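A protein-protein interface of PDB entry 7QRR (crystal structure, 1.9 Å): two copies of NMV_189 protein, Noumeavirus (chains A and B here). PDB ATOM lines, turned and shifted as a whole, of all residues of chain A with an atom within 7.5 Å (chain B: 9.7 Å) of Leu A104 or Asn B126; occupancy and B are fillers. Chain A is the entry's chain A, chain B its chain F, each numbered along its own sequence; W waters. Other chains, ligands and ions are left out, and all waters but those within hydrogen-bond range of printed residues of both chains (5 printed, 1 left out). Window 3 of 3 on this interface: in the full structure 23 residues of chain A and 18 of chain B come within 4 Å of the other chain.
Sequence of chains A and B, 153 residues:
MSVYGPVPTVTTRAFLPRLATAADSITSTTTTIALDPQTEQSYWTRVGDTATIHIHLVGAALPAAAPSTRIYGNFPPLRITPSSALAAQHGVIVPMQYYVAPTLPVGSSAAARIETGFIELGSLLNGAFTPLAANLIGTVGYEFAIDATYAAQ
7 positions are printed for both chains.
Water W5 bridges OD1 of Asn B126 (2.5 Å) and O of Ser A108 (2.8 Å). Water W2 lies within hydrogen-bond range of the backbone carbonyl oxygen of Pro A102 (2.7 Å) and the side-chain amide nitrogen of Asn B126 (3.4 Å). Water W4 lies within hydrogen-bond range of N of Asn B126 (2.8 Å) and O of Ser A108 (2.9 Å). Water W3 lies within hydrogen-bond range of NE2 of Gln A97 (2.9 Å) and N of Phe B129 (2.9 Å). Water W1 bridges N of Ile B93 (3.0 Å) and OE1 of Gln A97 (3.0 Å).
Among the printed residues, merely in contact across the chains: Gln A97 with Ile B93 (3.3 Å), Gln A97 with Gly B127 (3.4 Å), Pro A102 with Asn B126 (3.6 Å), Leu A104 with Asn B126 (3.7 Å), Ala A110 with Gly B127 (3.7 Å), Met A96 with Gly B127 (3.7 Å), Tyr A98 with Ala B128 (3.9 Å) and Tyr A98 with Asn B126 (3.96 Å).
The backbone carbonyl oxygen of Gly B127 is in hydrogen-bond range of the backbone NH of Tyr A98 (2.9 Å).
Printed residues of chain A that touch a printed residue of chain B: Met A96, Gln A97, Tyr A98, Pro A102, Leu A104 and Ala A110. Hydrophobic or aromatic side chains of chain A that line the printed part of chain B: Tyr A98, Pro A102, Leu A104 and Ala A110. Hydrophobic or aromatic side chains of chain B that line the printed part of chain A: Ile B93. Among the printed residues, 9 pairs touch across the chains. Among the printed residues, no Asp or Glu carboxylate lies within 4 Å of a Lys or Arg side-chain nitrogen of the other chain.
The backbone carbonyl oxygen (O) of Ala A110 is in hydrogen-bond range of the backbone NH (N) of Met A96, 3.2 Å away. The side-chain amide oxygen (OE1) of Gln A97 is in hydrogen-bond range of the side-chain hydroxyl (OH) of Tyr A99 (3.4 Å).
Of chain B, only Asn B126 (3.7 Å) comes within 4 Å of Leu A104. No residue of chain B comes within 4 Å of Pro A105. Printed residues of chain A within 4 Å of Ile B93: Gln A97. Printed residues of chain B within 4 Å of Met A96: Gly B127 (3.7 Å). Printed residues of chain B within 4 Å of Tyr A98: Asn B126 (3.96 Å), Gly B127 (2.9 Å) and Ala B128 (3.9 Å). The nearest residue of chain B that does not touch Leu A104 is Gly B127 (5.0 Å).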
ATOM      1  N   MET A  96       3.292 -33.430 -28.017  1.00  0.00           N
ATOM      2  CA  MET A  96       2.170 -34.087 -27.355  1.00  0.00           C
ATOM      3  C   MET A  96       1.282 -33.036 -26.706  1.00  0.00           C
ATOM      4  O   MET A  96       1.648 -31.870 -26.634  1.00  0.00           O
ATOM      5  CB  MET A  96       2.644 -35.122 -26.325  1.00  0.00           C
ATOM      6  CG  MET A  96       3.470 -34.566 -25.161  1.00  0.00           C
ATOM      7  SD  MET A  96       3.871 -35.860 -23.947  1.00  0.00           S
ATOM      8  CE  MET A  96       2.262 -36.098 -23.173  1.00  0.00           C
ATOM      9  N   GLN A  97       0.112 -33.471 -26.252  1.00  0.00           N
ATOM     10  CA  GLN A  97      -0.908 -32.563 -25.760  1.00  0.00           C
ATOM     11  C   GLN A  97      -1.128 -32.747 -24.264  1.00  0.00           C
ATOM     12  O   GLN A  97      -1.166 -33.873 -23.774  1.00  0.00           O
ATOM     13  CB  GLN A  97      -2.220 -32.782 -26.528  1.00  0.00           C
ATOM     14  CG  GLN A  97      -3.349 -31.858 -26.067  1.00  0.00           C
ATOM     15  CD  GLN A  97      -4.630 -32.076 -26.834  1.00  0.00           C
ATOM     16  OE1 GLN A  97      -4.775 -33.060 -27.582  1.00  0.00           O
ATOM     17  NE2 GLN A  97      -5.568 -31.160 -26.667  1.00  0.00           N
ATOM     18  N   TYR A  98      -1.260 -31.637 -23.539  1.00  0.00           N
ATOM     19  CA  TYR A  98      -1.611 -31.667 -22.121  1.00  0.00           C
ATOM     20  C   TYR A  98      -2.956 -30.990 -21.885  1.00  0.00           C
ATOM     21  O   TYR A  98      -3.152 -29.837 -22.284  1.00  0.00           O
ATOM     22  CB  TYR A  98      -0.534 -30.970 -21.267  1.00  0.00           C
ATOM     23  CG  TYR A  98       0.666 -31.839 -20.974  1.00  0.00           C
ATOM     24  CD1 TYR A  98       0.624 -32.798 -19.959  1.00  0.00           C
ATOM     25  CD2 TYR A  98       1.841 -31.711 -21.711  1.00  0.00           C
ATOM     26  CE1 TYR A  98       1.719 -33.602 -19.683  1.00  0.00           C
ATOM     27  CE2 TYR A  98       2.952 -32.526 -21.446  1.00  0.00           C
ATOM     28  CZ  TYR A  98       2.881 -33.462 -20.430  1.00  0.00           C
ATOM     29  OH  TYR A  98       3.965 -34.265 -20.145  1.00  0.00           O
ATOM     30  N   TYR A  99      -3.867 -31.698 -21.222  1.00  0.00           N
ATOM     31  CA  TYR A  99      -5.124 -31.101 -20.769  1.00  0.00           C
ATOM     32  C   TYR A  99      -5.027 -30.513 -19.357  1.00  0.00           C
ATOM     33  O   TYR A  99      -5.834 -29.673 -18.964  1.00  0.00           O
ATOM     34  CB  TYR A  99      -6.241 -32.142 -20.799  1.00  0.00           C
ATOM     35  CG  TYR A  99      -6.594 -32.627 -22.184  1.00  0.00           C
ATOM     36  CD1 TYR A  99      -7.564 -31.977 -22.938  1.00  0.00           C
ATOM     37  CD2 TYR A  99      -5.961 -33.736 -22.736  1.00  0.00           C
ATOM     38  CE1 TYR A  99      -7.906 -32.421 -24.207  1.00  0.00           C
ATOM     39  CE2 TYR A  99      -6.292 -34.191 -24.013  1.00  0.00           C
ATOM     40  CZ  TYR A  99      -7.268 -33.528 -24.738  1.00  0.00           C
ATOM     41  OH  TYR A  99      -7.621 -33.967 -25.995  1.00  0.00           O
ATOM     42  N   VAL A 100      -4.065 -31.000 -18.584  1.00  0.00           N
ATOM     43  CA  VAL A 100      -3.730 -30.415 -17.292  1.00  0.00           C
ATOM     44  C   VAL A 100      -2.275 -29.966 -17.393  1.00  0.00           C
ATOM     45  O   VAL A 100      -1.441 -30.721 -17.883  1.00  0.00           O
ATOM     46  CB  VAL A 100      -3.918 -31.426 -16.138  1.00  0.00           C
ATOM     47  CG1 VAL A 100      -3.414 -30.848 -14.813  1.00  0.00           C
ATOM     48  CG2 VAL A 100      -5.377 -31.853 -16.025  1.00  0.00           C
ATOM     49  N   ALA A 101      -1.970 -28.745 -16.959  1.00  0.00           N
ATOM     50  CA  ALA A 101      -0.659 -28.162 -17.247  1.00  0.00           C
ATOM     51  C   ALA A 101       0.483 -28.872 -16.524  1.00  0.00           C
ATOM     52  O   ALA A 101       0.388 -29.186 -15.336  1.00  0.00           O
ATOM     53  CB  ALA A 101      -0.643 -26.687 -16.898  1.00  0.00           C
ATOM     54  N   PRO A 102       1.579 -29.115 -17.255  1.00  0.00           N
ATOM     55  CA  PRO A 102       2.807 -29.674 -16.704  1.00  0.00           C
ATOM     56  C   PRO A 102       3.735 -28.547 -16.276  1.00  0.00           C
ATOM     57  O   PRO A 102       3.371 -27.368 -16.393  1.00  0.00           O
ATOM     58  CB  PRO A 102       3.390 -30.445 -17.894  1.00  0.00           C
ATOM     59  CG  PRO A 102       3.034 -29.549 -19.089  1.00  0.00           C
ATOM     60  CD  PRO A 102       1.689 -28.879 -18.710  1.00  0.00           C
ATOM     61  N   THR A 103       4.919 -28.899 -15.793  1.00  0.00           N
ATOM     62  CA  THR A 103       5.986 -27.917 -15.632  1.00  0.00           C
ATOM     63  C   THR A 103       7.120 -28.278 -16.573  1.00  0.00           C
ATOM     64  O   THR A 103       7.780 -29.294 -16.373  1.00  0.00           O
ATOM     65  CB  THR A 103       6.515 -27.871 -14.179  1.00  0.00           C
ATOM     66  OG1 THR A 103       5.452 -27.506 -13.296  1.00  0.00           O
ATOM     67  CG2 THR A 103       7.655 -26.863 -14.050  1.00  0.00           C
ATOM     68  N   LEU A 104       7.345 -27.447 -17.594  1.00  0.00           N
ATOM     69  CA  LEU A 104       8.379 -27.702 -18.602  1.00  0.00           C
ATOM     70  C   LEU A 104       9.516 -26.703 -18.474  1.00  0.00           C
ATOM     71  O   LEU A 104       9.325 -25.618 -17.911  1.00  0.00           O
ATOM     72  CB  LEU A 104       7.794 -27.611 -20.031  1.00  0.00           C
ATOM     73  CG  LEU A 104       6.569 -28.447 -20.417  1.00  0.00           C
ATOM     74  CD1 LEU A 104       6.248 -28.234 -21.903  1.00  0.00           C
ATOM     75  CD2 LEU A 104       6.766 -29.941 -20.129  1.00  0.00           C
ATOM     76  N   PRO A 105      10.696 -27.053 -19.006  1.00  0.00           N
ATOM     77  CA  PRO A 105      11.799 -26.084 -19.036  1.00  0.00           C
ATOM     78  C   PRO A 105      11.414 -24.843 -19.844  1.00  0.00           C
ATOM     79  O   PRO A 105      10.650 -24.945 -20.809  1.00  0.00           O
ATOM     80  CB  PRO A 105      12.933 -26.868 -19.693  1.00  0.00           C
ATOM     81  CG  PRO A 105      12.615 -28.331 -19.352  1.00  0.00           C
ATOM     82  CD  PRO A 105      11.122 -28.407 -19.425  1.00  0.00           C
ATOM     83  N   VAL A 106      11.928 -23.682 -19.441  1.00  0.00           N
ATOM     84  CA  VAL A 106      11.584 -22.433 -20.114  1.00  0.00           C
ATOM     85  C   VAL A 106      11.891 -22.524 -21.611  1.00  0.00           C
ATOM     86  O   VAL A 106      12.920 -23.068 -22.018  1.00  0.00           O
ATOM     87  CB  VAL A 106      12.331 -21.219 -19.487  1.00  0.00           C
ATOM     88  CG1 VAL A 106      13.836 -21.394 -19.576  1.00  0.00           C
ATOM     89  CG2 VAL A 106      11.897 -19.920 -20.147  1.00  0.00           C
ATOM     90  N   GLY A 107      10.966 -22.035 -22.428  1.00  0.00           N
ATOM     91  CA  GLY A 107      11.178 -22.000 -23.862  1.00  0.00           C
ATOM     92  C   GLY A 107      10.909 -23.306 -24.591  1.00  0.00           C
ATOM     93  O   GLY A 107      10.897 -23.326 -25.822  1.00  0.00           O
ATOM     94  N   SER A 108      10.678 -24.389 -23.851  1.00  0.00           N
ATOM     95  CA  SER A 108      10.508 -25.702 -24.489  1.00  0.00           C
ATOM     96  C   SER A 108       9.050 -26.009 -24.825  1.00  0.00           C
ATOM     97  O   SER A 108       8.132 -25.380 -24.283  1.00  0.00           O
ATOM     98  CB  SER A 108      11.071 -26.812 -23.598  1.00  0.00           C
ATOM     99  OG  SER A 108      10.260 -27.009 -22.454  1.00  0.00           O
ATOM    100  N   SER A 109       8.852 -26.977 -25.724  1.00  0.00           N
ATOM    101  CA  SER A 109       7.520 -27.467 -26.071  1.00  0.00           C
ATOM    102  C   SER A 109       7.309 -28.880 -25.508  1.00  0.00           C
ATOM    103  O   SER A 109       8.266 -29.607 -25.272  1.00  0.00           O
ATOM    104  CB  SER A 109       7.314 -27.466 -27.603  1.00  0.00           C
ATOM    105  OG  SER A 109       8.277 -28.280 -28.268  1.00  0.00           O
ATOM    106  N   ALA A 110       6.051 -29.249 -25.287  1.00  0.00           N
ATOM    107  CA  ALA A 110       5.696 -30.579 -24.818  1.00  0.00           C
ATOM    108  C   ALA A 110       5.998 -31.606 -25.900  1.00  0.00           C
ATOM    109  O   ALA A 110       5.593 -31.431 -27.054  1.00  0.00           O
ATOM    110  CB  ALA A 110       4.219 -30.632 -24.431  1.00  0.00           C
ATOM    111  N   ALA A 111       6.684 -32.686 -25.527  1.00  0.00           N
ATOM    112  CA  ALA A 111       7.117 -33.668 -26.531  1.00  0.00           C
ATOM    113  C   ALA A 111       7.150 -35.082 -25.975  1.00  0.00           C
ATOM    114  O   ALA A 111       7.098 -35.293 -24.760  1.00  0.00           O
ATOM    115  CB  ALA A 111       8.502 -33.303 -27.078  1.00  0.00           C
ATOM    116  N   GLY A 122       8.608 -35.904 -22.467  1.00  0.00           N
ATOM    117  CA  GLY A 122       9.640 -34.913 -22.215  1.00  0.00           C
ATOM    118  C   GLY A 122       9.338 -33.539 -22.773  1.00  0.00           C
ATOM    119  O   GLY A 122       8.180 -33.134 -22.908  1.00  0.00           O
ATOM    120  N   SER A 123      10.400 -32.819 -23.104  1.00  0.00           N
ATOM    121  CA  SER A 123      10.254 -31.486 -23.650  1.00  0.00           C
ATOM    122  C   SER A 123      11.288 -31.279 -24.754  1.00  0.00           C
ATOM    123  O   SER A 123      12.287 -31.997 -24.830  1.00  0.00           O
ATOM    124  CB  SER A 123      10.393 -30.433 -22.545  1.00  0.00           C
ATOM    125  OG  SER A 123      11.718 -30.432 -22.016  1.00  0.00           O
ATOM    126  N   LEU A 124      11.053 -30.282 -25.601  1.00  0.00           N
ATOM    127  CA  LEU A 124      11.810 -30.129 -26.831  1.00  0.00           C
ATOM    128  C   LEU A 124      12.278 -28.696 -26.981  1.00  0.00           C
ATOM    129  O   LEU A 124      11.470 -27.777 -26.895  1.00  0.00           O
ATOM    130  CB  LEU A 124      10.950 -30.537 -28.035  1.00  0.00           C
ATOM    131  CG  LEU A 124      11.541 -30.401 -29.436  1.00  0.00           C
ATOM    132  CD1 LEU A 124      12.793 -31.252 -29.594  1.00  0.00           C
ATOM    133  CD2 LEU A 124      10.487 -30.797 -30.497  1.00  0.00           C
ATOM    134  N   THR A 130      14.565 -33.575 -23.956  1.00  0.00           N
ATOM    135  CA  THR A 130      14.900 -33.753 -22.541  1.00  0.00           C
ATOM    136  C   THR A 130      13.763 -34.488 -21.831  1.00  0.00           C
ATOM    137  O   THR A 130      12.624 -34.035 -21.895  1.00  0.00           O
ATOM    138  CB  THR A 130      15.129 -32.379 -21.844  1.00  0.00           C
ATOM    139  OG1 THR A 130      16.202 -31.687 -22.488  1.00  0.00           O
ATOM    140  CG2 THR A 130      15.460 -32.546 -20.373  1.00  0.00           C
ATOM    141  N   LEU A 132      11.091 -35.689 -19.077  1.00  0.00           N
ATOM    142  CA  LEU A 132      10.373 -34.937 -18.051  1.00  0.00           C
ATOM    143  C   LEU A 132      10.125 -35.806 -16.816  1.00  0.00           C
ATOM    144  O   LEU A 132       9.646 -36.931 -16.937  1.00  0.00           O
ATOM    145  CB  LEU A 132       9.040 -34.425 -18.605  1.00  0.00           C
ATOM    146  CG  LEU A 132       8.181 -33.522 -17.708  1.00  0.00           C
ATOM    147  CD1 LEU A 132       8.947 -32.249 -17.350  1.00  0.00           C
ATOM    148  CD2 LEU A 132       6.856 -33.178 -18.407  1.00  0.00           C
ATOM    149  N   LEU A 136       6.209 -33.886 -12.666  1.00  0.00           N
ATOM    150  CA  LEU A 136       6.039 -32.623 -13.384  1.00  0.00           C
ATOM    151  C   LEU A 136       5.105 -32.759 -14.589  1.00  0.00           C
ATOM    152  O   LEU A 136       4.956 -31.810 -15.359  1.00  0.00           O
ATOM    153  CB  LEU A 136       7.402 -32.088 -13.847  1.00  0.00           C
ATOM    154  CG  LEU A 136       8.407 -31.807 -12.720  1.00  0.00           C
ATOM    155  CD1 LEU A 136       9.680 -31.191 -13.265  1.00  0.00           C
ATOM    156  CD2 LEU A 136       7.797 -30.896 -11.652  1.00  0.00           C
ATOM    157  N   ILE A 137       4.461 -33.918 -14.743  1.00  0.00           N
ATOM    158  CA  ILE A 137       3.651 -34.159 -15.948  1.00  0.00           C
ATOM    159  C   ILE A 137       2.222 -33.650 -15.783  1.00  0.00           C
ATOM    160  O   ILE A 137       1.318 -34.026 -16.534  1.00  0.00           O
ATOM    161  CB  ILE A 137       3.611 -35.667 -16.326  1.00  0.00           C
ATOM    162  CG1 ILE A 137       2.920 -36.471 -15.229  1.00  0.00           C
ATOM    163  CG2 ILE A 137       5.014 -36.195 -16.615  1.00  0.00           C
ATOM    164  CD1 ILE A 137       2.684 -37.945 -15.601  1.00  0.00           C
ATOM    165  N   ILE B  93      -3.810 -32.493 -31.766  1.00  0.00           N
ATOM    166  CA  ILE B  93      -3.171 -31.195 -32.036  1.00  0.00           C
ATOM    167  C   ILE B  93      -1.976 -31.372 -32.959  1.00  0.00           C
ATOM    168  O   ILE B  93      -1.091 -32.188 -32.690  1.00  0.00           O
ATOM    169  CB  ILE B  93      -2.685 -30.495 -30.738  1.00  0.00           C
ATOM    170  CG1 ILE B  93      -3.782 -30.508 -29.663  1.00  0.00           C
ATOM    171  CG2 ILE B  93      -2.195 -29.068 -31.059  1.00  0.00           C
ATOM    172  CD1 ILE B  93      -5.112 -29.884 -30.092  1.00  0.00           C
ATOM    173  N   VAL B 106       2.225 -14.792 -27.147  1.00  0.00           N
ATOM    174  CA  VAL B 106       3.676 -14.825 -26.956  1.00  0.00           C
ATOM    175  C   VAL B 106       4.145 -16.218 -26.542  1.00  0.00           C
ATOM    176  O   VAL B 106       3.525 -16.860 -25.699  1.00  0.00           O
ATOM    177  CB  VAL B 106       4.133 -13.802 -25.892  1.00  0.00           C
ATOM    178  CG1 VAL B 106       5.620 -13.944 -25.611  1.00  0.00           C
ATOM    179  CG2 VAL B 106       3.804 -12.392 -26.348  1.00  0.00           C
ATOM    180  N   GLY B 107       5.217 -16.694 -27.166  1.00  0.00           N
ATOM    181  CA  GLY B 107       5.773 -17.990 -26.824  1.00  0.00           C
ATOM    182  C   GLY B 107       5.078 -19.190 -27.448  1.00  0.00           C
ATOM    183  O   GLY B 107       5.581 -20.298 -27.330  1.00  0.00           O
ATOM    184  N   SER B 108       3.934 -18.986 -28.100  1.00  0.00           N
ATOM    185  CA  SER B 108       3.181 -20.120 -28.641  1.00  0.00           C
ATOM    186  C   SER B 108       3.590 -20.458 -30.078  1.00  0.00           C
ATOM    187  O   SER B 108       4.188 -19.635 -30.774  1.00  0.00           O
ATOM    188  CB  SER B 108       1.675 -19.844 -28.584  1.00  0.00           C
ATOM    189  OG  SER B 108       1.299 -18.874 -29.550  1.00  0.00           O
ATOM    190  N   SER B 109       3.262 -21.672 -30.522  1.00  0.00           N
ATOM    191  CA  SER B 109       3.479 -22.055 -31.920  1.00  0.00           C
ATOM    192  C   SER B 109       2.140 -22.156 -32.659  1.00  0.00           C
ATOM    193  O   SER B 109       1.103 -22.365 -32.035  1.00  0.00           O
ATOM    194  CB  SER B 109       4.220 -23.396 -32.008  1.00  0.00           C
ATOM    195  OG  SER B 109       3.485 -24.395 -31.306  1.00  0.00           O
ATOM    196  N   SER B 123      -3.278 -22.021 -31.351  1.00  0.00           N
ATOM    197  CA  SER B 123      -1.875 -21.932 -30.976  1.00  0.00           C
ATOM    198  C   SER B 123      -1.590 -22.923 -29.844  1.00  0.00           C
ATOM    199  O   SER B 123      -2.510 -23.411 -29.174  1.00  0.00           O
ATOM    200  CB  SER B 123      -1.504 -20.500 -30.559  1.00  0.00           C
ATOM    201  OG  SER B 123      -2.204 -20.108 -29.382  1.00  0.00           O
ATOM    202  N   LEU B 124      -0.309 -23.203 -29.634  1.00  0.00           N
ATOM    203  CA  LEU B 124       0.115 -24.284 -28.763  1.00  0.00           C
ATOM    204  C   LEU B 124       1.188 -23.795 -27.797  1.00  0.00           C
ATOM    205  O   LEU B 124       2.204 -23.253 -28.219  1.00  0.00           O
ATOM    206  CB  LEU B 124       0.641 -25.457 -29.598  1.00  0.00           C
ATOM    207  CG  LEU B 124       1.143 -26.720 -28.900  1.00  0.00           C
ATOM    208  CD1 LEU B 124       0.066 -27.310 -27.999  1.00  0.00           C
ATOM    209  CD2 LEU B 124       1.603 -27.742 -29.961  1.00  0.00           C
ATOM    210  N   LEU B 125       0.952 -23.992 -26.507  1.00  0.00           N
ATOM    211  CA  LEU B 125       1.899 -23.549 -25.486  1.00  0.00           C
ATOM    212  C   LEU B 125       1.856 -24.515 -24.318  1.00  0.00           C
ATOM    213  O   LEU B 125       0.781 -24.743 -23.744  1.00  0.00           O
ATOM    214  CB  LEU B 125       1.564 -22.114 -25.036  1.00  0.00           C
ATOM    215  CG  LEU B 125       2.480 -21.485 -23.978  1.00  0.00           C
ATOM    216  CD1 LEU B 125       3.853 -21.261 -24.547  1.00  0.00           C
ATOM    217  CD2 LEU B 125       1.879 -20.171 -23.460  1.00  0.00           C
ATOM    218  N   ASN B 126       3.014 -25.098 -23.991  1.00  0.00           N
ATOM    219  CA  ASN B 126       3.118 -26.098 -22.920  1.00  0.00           C
ATOM    220  C   ASN B 126       2.120 -27.233 -23.092  1.00  0.00           C
ATOM    221  O   ASN B 126       1.522 -27.701 -22.123  1.00  0.00           O
ATOM    222  CB  ASN B 126       2.926 -25.436 -21.553  1.00  0.00           C
ATOM    223  CG  ASN B 126       4.008 -24.448 -21.255  1.00  0.00           C
ATOM    224  OD1 ASN B 126       5.185 -24.761 -21.420  1.00  0.00           O
ATOM    225  ND2 ASN B 126       3.630 -23.243 -20.831  1.00  0.00           N
ATOM    226  N   GLY B 127       1.946 -27.675 -24.333  1.00  0.00           N
ATOM    227  CA  GLY B 127       1.039 -28.777 -24.609  1.00  0.00           C
ATOM    228  C   GLY B 127      -0.427 -28.389 -24.702  1.00  0.00           C
ATOM    229  O   GLY B 127      -1.248 -29.221 -25.066  1.00  0.00           O
ATOM    230  N   ALA B 128      -0.764 -27.138 -24.377  1.00  0.00           N
ATOM    231  CA  ALA B 128      -2.173 -26.708 -24.375  1.00  0.00           C
ATOM    232  C   ALA B 128      -2.562 -25.983 -25.662  1.00  0.00           C
ATOM    233  O   ALA B 128      -1.858 -25.071 -26.100  1.00  0.00           O
ATOM    234  CB  ALA B 128      -2.464 -25.800 -23.168  1.00  0.00           C
ATOM    235  N   PHE B 129      -3.694 -26.382 -26.248  1.00  0.00           N
ATOM    236  CA  PHE B 129      -4.216 -25.738 -27.455  1.00  0.00           C
ATOM    237  C   PHE B 129      -5.173 -24.604 -27.100  1.00  0.00           C
ATOM    238  O   PHE B 129      -6.065 -24.786 -26.270  1.00  0.00           O
ATOM    239  CB  PHE B 129      -4.938 -26.758 -28.344  1.00  0.00           C
ATOM    240  CG  PHE B 129      -5.537 -26.160 -29.587  1.00  0.00           C
ATOM    241  CD1 PHE B 129      -4.772 -26.017 -30.742  1.00  0.00           C
ATOM    242  CD2 PHE B 129      -6.870 -25.744 -29.606  1.00  0.00           C
ATOM    243  CE1 PHE B 129      -5.326 -25.469 -31.894  1.00  0.00           C
ATOM    244  CE2 PHE B 129      -7.423 -25.180 -30.745  1.00  0.00           C
ATOM    245  CZ  PHE B 129      -6.652 -25.049 -31.891  1.00  0.00           C
ATOM    246  N   THR B 130      -4.980 -23.440 -27.720  1.00  0.00           N
ATOM    247  CA  THR B 130      -5.874 -22.286 -27.545  1.00  0.00           C
ATOM    248  C   THR B 130      -6.409 -21.845 -28.912  1.00  0.00           C
ATOM    249  O   THR B 130      -5.623 -21.586 -29.814  1.00  0.00           O
ATOM    250  CB  THR B 130      -5.148 -21.094 -26.884  1.00  0.00           C
ATOM    251  OG1 THR B 130      -4.741 -21.462 -25.565  1.00  0.00           O
ATOM    252  CG2 THR B 130      -6.066 -19.877 -26.803  1.00  0.00           C
HETATM  253  O   HOH W   1      -2.873 -34.347 -29.578  1.00  0.00           O
HETATM  254  O   HOH W   2       3.075 -25.367 -18.224  1.00  0.00           O
HETATM  255  O   HOH W   3      -5.168 -28.697 -25.182  1.00  0.00           O
HETATM  256  O   HOH W   4       5.494 -24.504 -25.214  1.00  0.00           O
HETATM  257  O   HOH W   5       7.444 -23.847 -21.987  1.00  0.00           O
